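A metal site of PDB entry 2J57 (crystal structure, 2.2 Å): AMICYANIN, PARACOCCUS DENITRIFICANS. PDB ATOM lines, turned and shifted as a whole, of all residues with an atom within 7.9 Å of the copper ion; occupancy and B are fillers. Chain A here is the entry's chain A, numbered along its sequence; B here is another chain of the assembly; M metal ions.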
ATOM      1  N   ILE A  25     -24.332 -11.152 -32.506  1.00  0.00           N
ATOM      2  CA  ILE A  25     -23.543 -11.811 -31.491  1.00  0.00           C
ATOM      3  C   ILE A  25     -24.023 -13.233 -31.221  1.00  0.00           C
ATOM      4  O   ILE A  25     -25.182 -13.443 -30.855  1.00  0.00           O
ATOM      5  CB  ILE A  25     -23.422 -10.974 -30.131  1.00  0.00           C
ATOM      6  CG1 ILE A  25     -23.273  -9.462 -30.390  1.00  0.00           C
ATOM      7  CG2 ILE A  25     -22.268 -11.495 -29.285  1.00  0.00           C
ATOM      8  CD1 ILE A  25     -23.599  -8.577 -29.158  1.00  0.00           C
ATOM      9  N   MET A  28     -20.147 -16.788 -28.421  1.00  0.00           N
ATOM     10  CA  MET A  28     -19.103 -16.055 -27.669  1.00  0.00           C
ATOM     11  C   MET A  28     -18.269 -15.205 -28.635  1.00  0.00           C
ATOM     12  O   MET A  28     -17.068 -14.972 -28.422  1.00  0.00           O
ATOM     13  CB  MET A  28     -18.226 -17.028 -26.865  1.00  0.00           C
ATOM     14  CG  MET A  28     -19.055 -17.984 -25.940  1.00  0.00           C
ATOM     15  SD  MET A  28     -20.146 -17.039 -24.830  1.00  0.00           S
ATOM     16  CE  MET A  28     -18.907 -16.310 -23.768  1.00  0.00           C
ATOM     17  N   LYS A  29     -18.932 -14.724 -29.713  1.00  0.00           N
ATOM     18  CA  LYS A  29     -18.257 -13.891 -30.701  1.00  0.00           C
ATOM     19  C   LYS A  29     -19.075 -12.710 -31.238  1.00  0.00           C
ATOM     20  O   LYS A  29     -20.282 -12.797 -31.483  1.00  0.00           O
ATOM     21  CB  LYS A  29     -17.794 -14.727 -31.882  1.00  0.00           C
ATOM     22  CG  LYS A  29     -16.548 -15.530 -31.674  1.00  0.00           C
ATOM     23  CD  LYS A  29     -16.419 -16.576 -32.807  1.00  0.00           C
ATOM     24  CE  LYS A  29     -15.262 -17.547 -32.524  1.00  0.00           C
ATOM     25  NZ  LYS A  29     -14.579 -17.979 -33.805  1.00  0.00           N
ATOM     26  N   TYR A  30     -18.394 -11.614 -31.481  1.00  0.00           N
ATOM     27  CA  TYR A  30     -18.963 -10.611 -32.340  1.00  0.00           C
ATOM     28  C   TYR A  30     -18.781 -11.160 -33.753  1.00  0.00           C
ATOM     29  O   TYR A  30     -17.670 -11.532 -34.142  1.00  0.00           O
ATOM     30  CB  TYR A  30     -18.232  -9.331 -32.151  1.00  0.00           C
ATOM     31  CG  TYR A  30     -18.335  -8.748 -30.759  1.00  0.00           C
ATOM     32  CD1 TYR A  30     -19.547  -8.254 -30.295  1.00  0.00           C
ATOM     33  CD2 TYR A  30     -17.196  -8.632 -29.928  1.00  0.00           C
ATOM     34  CE1 TYR A  30     -19.637  -7.694 -29.024  1.00  0.00           C
ATOM     35  CE2 TYR A  30     -17.277  -8.076 -28.694  1.00  0.00           C
ATOM     36  CZ  TYR A  30     -18.488  -7.607 -28.228  1.00  0.00           C
ATOM     37  OH  TYR A  30     -18.597  -7.035 -26.978  1.00  0.00           O
ATOM     38  N   ASN A  47     -27.832  -9.374 -30.002  1.00  0.00           N
ATOM     39  CA  ASN A  47     -27.498 -10.654 -29.379  1.00  0.00           C
ATOM     40  C   ASN A  47     -28.404 -11.805 -29.826  1.00  0.00           C
ATOM     41  O   ASN A  47     -29.599 -11.790 -29.563  1.00  0.00           O
ATOM     42  CB  ASN A  47     -27.469 -10.501 -27.838  1.00  0.00           C
ATOM     43  CG  ASN A  47     -26.824 -11.666 -27.144  1.00  0.00           C
ATOM     44  OD1 ASN A  47     -26.279 -12.560 -27.777  1.00  0.00           O
ATOM     45  ND2 ASN A  47     -26.867 -11.659 -25.807  1.00  0.00           N
ATOM     46  N   GLU A  49     -28.017 -15.064 -28.807  1.00  0.00           N
ATOM     47  CA  GLU A  49     -27.952 -16.194 -27.839  1.00  0.00           C
ATOM     48  C   GLU A  49     -28.391 -15.786 -26.421  1.00  0.00           C
ATOM     49  O   GLU A  49     -28.565 -14.569 -26.119  1.00  0.00           O
ATOM     50  CB  GLU A  49     -26.568 -16.914 -27.822  1.00  0.00           C
ATOM     51  CG  GLU A  49     -25.315 -16.006 -27.653  1.00  0.00           C
ATOM     52  CD  GLU A  49     -24.030 -16.803 -27.534  1.00  0.00           C
ATOM     53  OE1 GLU A  49     -24.096 -18.029 -27.659  1.00  0.00           O
ATOM     54  OE2 GLU A  49     -22.974 -16.217 -27.298  1.00  0.00           O
ATOM     55  N   MET A  51     -26.776 -16.334 -23.632  1.00  0.00           N
ATOM     56  CA  MET A  51     -25.672 -15.679 -22.947  1.00  0.00           C
ATOM     57  C   MET A  51     -25.693 -14.144 -23.163  1.00  0.00           C
ATOM     58  O   MET A  51     -25.437 -13.716 -24.275  1.00  0.00           O
ATOM     59  CB  MET A  51     -24.341 -16.232 -23.456  1.00  0.00           C
ATOM     60  CG  MET A  51     -23.073 -15.603 -22.833  1.00  0.00           C
ATOM     61  SD  MET A  51     -22.797 -16.193 -21.152  1.00  0.00           S
ATOM     62  CE  MET A  51     -22.114 -17.842 -21.435  1.00  0.00           C
ATOM     63  N   PRO A  52     -25.945 -13.324 -22.099  1.00  0.00           N
ATOM     64  CA  PRO A  52     -25.822 -11.883 -22.268  1.00  0.00           C
ATOM     65  C   PRO A  52     -24.453 -11.364 -22.738  1.00  0.00           C
ATOM     66  O   PRO A  52     -23.411 -11.853 -22.329  1.00  0.00           O
ATOM     67  CB  PRO A  52     -26.137 -11.345 -20.858  1.00  0.00           C
ATOM     68  CG  PRO A  52     -27.088 -12.366 -20.296  1.00  0.00           C
ATOM     69  CD  PRO A  52     -26.366 -13.634 -20.707  1.00  0.00           C
ATOM     70  N   HIS A  53     -24.489 -10.341 -23.599  1.00  0.00           N
ATOM     71  CA  HIS A  53     -23.276  -9.700 -24.108  1.00  0.00           C
ATOM     72  C   HIS A  53     -23.478  -8.231 -24.137  1.00  0.00           C
ATOM     73  O   HIS A  53     -24.597  -7.778 -24.105  1.00  0.00           O
ATOM     74  CB  HIS A  53     -22.868 -10.207 -25.506  1.00  0.00           C
ATOM     75  CG  HIS A  53     -22.676 -11.691 -25.597  1.00  0.00           C
ATOM     76  ND1 HIS A  53     -21.631 -12.359 -24.978  1.00  0.00           N
ATOM     77  CD2 HIS A  53     -23.395 -12.635 -26.243  1.00  0.00           C
ATOM     78  CE1 HIS A  53     -21.704 -13.646 -25.272  1.00  0.00           C
ATOM     79  NE2 HIS A  53     -22.771 -13.849 -26.021  1.00  0.00           N
ATOM     80  N   ASN A  54     -22.381  -7.480 -24.207  1.00  0.00           N
ATOM     81  CA  ASN A  54     -22.451  -6.057 -24.409  1.00  0.00           C
ATOM     82  C   ASN A  54     -21.325  -5.579 -25.297  1.00  0.00           C
ATOM     83  O   ASN A  54     -20.552  -6.395 -25.816  1.00  0.00           O
ATOM     84  CB  ASN A  54     -22.478  -5.354 -23.034  1.00  0.00           C
ATOM     85  CG  ASN A  54     -21.066  -5.053 -22.436  1.00  0.00           C
ATOM     86  OD1 ASN A  54     -20.065  -5.814 -22.578  1.00  0.00           O
ATOM     87  ND2 ASN A  54     -21.010  -3.919 -21.697  1.00  0.00           N
ATOM     88  N   VAL A  55     -21.254  -4.263 -25.501  1.00  0.00           N
ATOM     89  CA  VAL A  55     -20.018  -3.642 -26.004  1.00  0.00           C
ATOM     90  C   VAL A  55     -19.461  -2.684 -24.934  1.00  0.00           C
ATOM     91  O   VAL A  55     -20.216  -2.138 -24.139  1.00  0.00           O
ATOM     92  CB  VAL A  55     -20.204  -2.945 -27.413  1.00  0.00           C
ATOM     93  CG1 VAL A  55     -20.561  -4.005 -28.483  1.00  0.00           C
ATOM     94  CG2 VAL A  55     -21.223  -1.799 -27.329  1.00  0.00           C
ATOM     95  N   MET A  71     -26.031  -4.845 -20.932  1.00  0.00           N
ATOM     96  CA  MET A  71     -26.002  -6.240 -21.345  1.00  0.00           C
ATOM     97  C   MET A  71     -27.278  -6.509 -22.111  1.00  0.00           C
ATOM     98  O   MET A  71     -28.386  -6.187 -21.629  1.00  0.00           O
ATOM     99  CB  MET A  71     -25.926  -7.172 -20.134  1.00  0.00           C
ATOM    100  CG  MET A  71     -24.579  -7.187 -19.352  1.00  0.00           C
ATOM    101  SD  MET A  71     -22.997  -7.304 -20.277  1.00  0.00           S
ATOM    102  CE  MET A  71     -22.917  -9.065 -20.521  1.00  0.00           C
ATOM    103  N   MET A  72     -27.097  -7.040 -23.319  1.00  0.00           N
ATOM    104  CA  MET A  72     -28.182  -7.438 -24.196  1.00  0.00           C
ATOM    105  C   MET A  72     -28.440  -8.886 -23.831  1.00  0.00           C
ATOM    106  O   MET A  72     -27.491  -9.702 -23.854  1.00  0.00           O
ATOM    107  CB  MET A  72     -27.729  -7.337 -25.664  1.00  0.00           C
ATOM    108  CG  MET A  72     -27.555  -5.906 -26.263  1.00  0.00           C
ATOM    109  SD  MET A  72     -26.514  -5.891 -27.792  1.00  0.00           S
ATOM    110  CE  MET A  72     -24.829  -5.926 -27.137  1.00  0.00           C
ATOM    111  N   HIS A  91     -14.812  -4.665 -26.521  1.00  0.00           N
ATOM    112  CA  HIS A  91     -14.728  -6.015 -25.995  1.00  0.00           C
ATOM    113  C   HIS A  91     -16.014  -6.210 -25.222  1.00  0.00           C
ATOM    114  O   HIS A  91     -16.794  -5.236 -25.083  1.00  0.00           O
ATOM    115  CB  HIS A  91     -13.513  -6.157 -25.093  1.00  0.00           C
ATOM    116  CG  HIS A  91     -13.664  -5.458 -23.764  1.00  0.00           C
ATOM    117  ND1 HIS A  91     -13.257  -4.156 -23.556  1.00  0.00           N
ATOM    118  CD2 HIS A  91     -14.152  -5.910 -22.582  1.00  0.00           C
ATOM    119  CE1 HIS A  91     -13.488  -3.837 -22.295  1.00  0.00           C
ATOM    120  NE2 HIS A  91     -14.064  -4.857 -21.695  1.00  0.00           N
ATOM    121  N   CYS A  92     -16.249  -7.445 -24.744  1.00  0.00           N
ATOM    122  CA  CYS A  92     -17.469  -7.700 -24.010  1.00  0.00           C
ATOM    123  C   CYS A  92     -17.139  -7.746 -22.517  1.00  0.00           C
ATOM    124  O   CYS A  92     -16.162  -8.420 -22.106  1.00  0.00           O
ATOM    125  CB  CYS A  92     -18.096  -8.981 -24.484  1.00  0.00           C
ATOM    126  SG  CYS A  92     -19.527  -9.426 -23.493  1.00  0.00           S
ATOM    127  N   THR A  93     -17.931  -7.042 -21.703  1.00  0.00           N
ATOM    128  CA  THR A  93     -17.478  -6.744 -20.315  1.00  0.00           C
ATOM    129  C   THR A  93     -17.089  -7.992 -19.456  1.00  0.00           C
ATOM    130  O   THR A  93     -16.020  -7.970 -18.864  1.00  0.00           O
ATOM    131  CB  THR A  93     -18.455  -5.852 -19.511  1.00  0.00           C
ATOM    132  OG1 THR A  93     -18.401  -4.549 -20.061  1.00  0.00           O
ATOM    133  CG2 THR A  93     -18.043  -5.789 -17.986  1.00  0.00           C
ATOM    134  N   PRO A  94     -17.981  -9.028 -19.360  1.00  0.00           N
ATOM    135  CA  PRO A  94     -17.613 -10.238 -18.600  1.00  0.00           C
ATOM    136  C   PRO A  94     -16.802 -11.189 -19.466  1.00  0.00           C
ATOM    137  O   PRO A  94     -16.271 -12.181 -18.980  1.00  0.00           O
ATOM    138  CB  PRO A  94     -18.971 -10.857 -18.228  1.00  0.00           C
ATOM    139  CG  PRO A  94     -19.854 -10.485 -19.392  1.00  0.00           C
ATOM    140  CD  PRO A  94     -19.350  -9.126 -19.889  1.00  0.00           C
ATOM    141  N   HIS A  95     -16.698 -10.879 -20.754  1.00  0.00           N
ATOM    142  CA  HIS A  95     -16.005 -11.791 -21.639  1.00  0.00           C
ATOM    143  C   HIS A  95     -14.923 -11.077 -22.367  1.00  0.00           C
ATOM    144  O   HIS A  95     -15.039 -10.860 -23.548  1.00  0.00           O
ATOM    145  CB  HIS A  95     -16.999 -12.491 -22.602  1.00  0.00           C
ATOM    146  CG  HIS A  95     -18.216 -13.079 -21.924  1.00  0.00           C
ATOM    147  ND1 HIS A  95     -19.427 -13.205 -22.571  1.00  0.00           N
ATOM    148  CD2 HIS A  95     -18.402 -13.572 -20.681  1.00  0.00           C
ATOM    149  CE1 HIS A  95     -20.320 -13.695 -21.731  1.00  0.00           C
ATOM    150  NE2 HIS A  95     -19.724 -13.943 -20.575  1.00  0.00           N
ATOM    151  N   PRO A  96     -13.858 -10.651 -21.658  1.00  0.00           N
ATOM    152  CA  PRO A  96     -12.972  -9.638 -22.306  1.00  0.00           C
ATOM    153  C   PRO A  96     -12.213 -10.254 -23.489  1.00  0.00           C
ATOM    154  O   PRO A  96     -11.383  -9.556 -24.131  1.00  0.00           O
ATOM    155  CB  PRO A  96     -11.969  -9.248 -21.172  1.00  0.00           C
ATOM    156  CG  PRO A  96     -12.510  -9.943 -19.866  1.00  0.00           C
ATOM    157  CD  PRO A  96     -13.359 -11.077 -20.319  1.00  0.00           C
ATOM    158  N   PHE A  97     -12.426 -11.572 -23.734  1.00  0.00           N
ATOM    159  CA  PHE A  97     -11.805 -12.292 -24.868  1.00  0.00           C
ATOM    160  C   PHE A  97     -12.630 -12.122 -26.152  1.00  0.00           C
ATOM    161  O   PHE A  97     -12.200 -12.511 -27.264  1.00  0.00           O
ATOM    162  CB  PHE A  97     -11.698 -13.802 -24.595  1.00  0.00           C
ATOM    163  CG  PHE A  97     -13.004 -14.434 -24.157  1.00  0.00           C
ATOM    164  CD1 PHE A  97     -13.932 -14.851 -25.097  1.00  0.00           C
ATOM    165  CD2 PHE A  97     -13.315 -14.551 -22.786  1.00  0.00           C
ATOM    166  CE1 PHE A  97     -15.116 -15.379 -24.693  1.00  0.00           C
ATOM    167  CE2 PHE A  97     -14.510 -15.088 -22.395  1.00  0.00           C
ATOM    168  CZ  PHE A  97     -15.411 -15.483 -23.345  1.00  0.00           C
ATOM    169  N   MET A  98     -13.849 -11.610 -25.971  1.00  0.00           N
ATOM    170  CA  MET A  98     -14.671 -11.134 -27.078  1.00  0.00           C
ATOM    171  C   MET A  98     -14.276  -9.686 -27.391  1.00  0.00           C
ATOM    172  O   MET A  98     -14.573  -8.764 -26.631  1.00  0.00           O
ATOM    173  CB  MET A  98     -16.138 -11.249 -26.711  1.00  0.00           C
ATOM    174  CG  MET A  98     -16.672 -12.680 -26.600  1.00  0.00           C
ATOM    175  SD  MET A  98     -18.320 -12.490 -25.955  1.00  0.00           S
ATOM    176  CE  MET A  98     -19.104 -11.676 -27.345  1.00  0.00           C
ATOM    177  N   GLU B 101     -17.170 -17.100 -18.299  1.00  0.00           N
ATOM    178  CA  GLU B 101     -18.595 -16.933 -18.660  1.00  0.00           C
ATOM    179  C   GLU B 101     -19.443 -17.767 -17.722  1.00  0.00           C
ATOM    180  O   GLU B 101     -20.615 -17.399 -17.441  1.00  0.00           O
ATOM    181  CB  GLU B 101     -18.834 -17.306 -20.142  1.00  0.00           C
ATOM    182  CG  GLU B 101     -18.498 -18.710 -20.566  1.00  0.00           C
ATOM    183  CD  GLU B 101     -17.209 -18.837 -21.323  1.00  0.00           C
ATOM    184  OE1 GLU B 101     -16.167 -18.164 -21.024  1.00  0.00           O
ATOM    185  OE2 GLU B 101     -17.211 -19.677 -22.238  1.00  0.00           O
HETATM  186 CU    CU M   1     -19.905 -11.575 -24.115  1.00  0.00          CU
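Merely in contact with the copper ion: Pro 52.
Five residues have an atom within 4 Å of the copper ion: Pro 52, His 53, Cys 92, His 95 and Met 98.
NE2 of His 53 is in hydrogen-bond range of OE2 of Glu 49, at 2.7 Å.
The backbone carbonyl oxygen of His 53 is in hydrogen-bond range of the backbone NH of Met 72, 2.7 Å away.
The backbone NH of Asn 54 sits close to the side-chain sulfur of Cys 92 (3.5 Å).
NE2 of His 53 sits close to O of Met 51.
The side-chain hydroxyl (OH) of Tyr 30 sits close to the backbone NH (N) of Cys 92 (3.3 Å).
The copper ion is bound by ND1 of His 53.
SG of Cys 92 is bound to the copper ion, at 2.3 Å.
ND1 of His 95 is bound to the copper ion (2.3 Å).
SD of Met 98 is bound to the copper ion (2.6 Å).
The copper ion has four donor atoms within binding distance.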
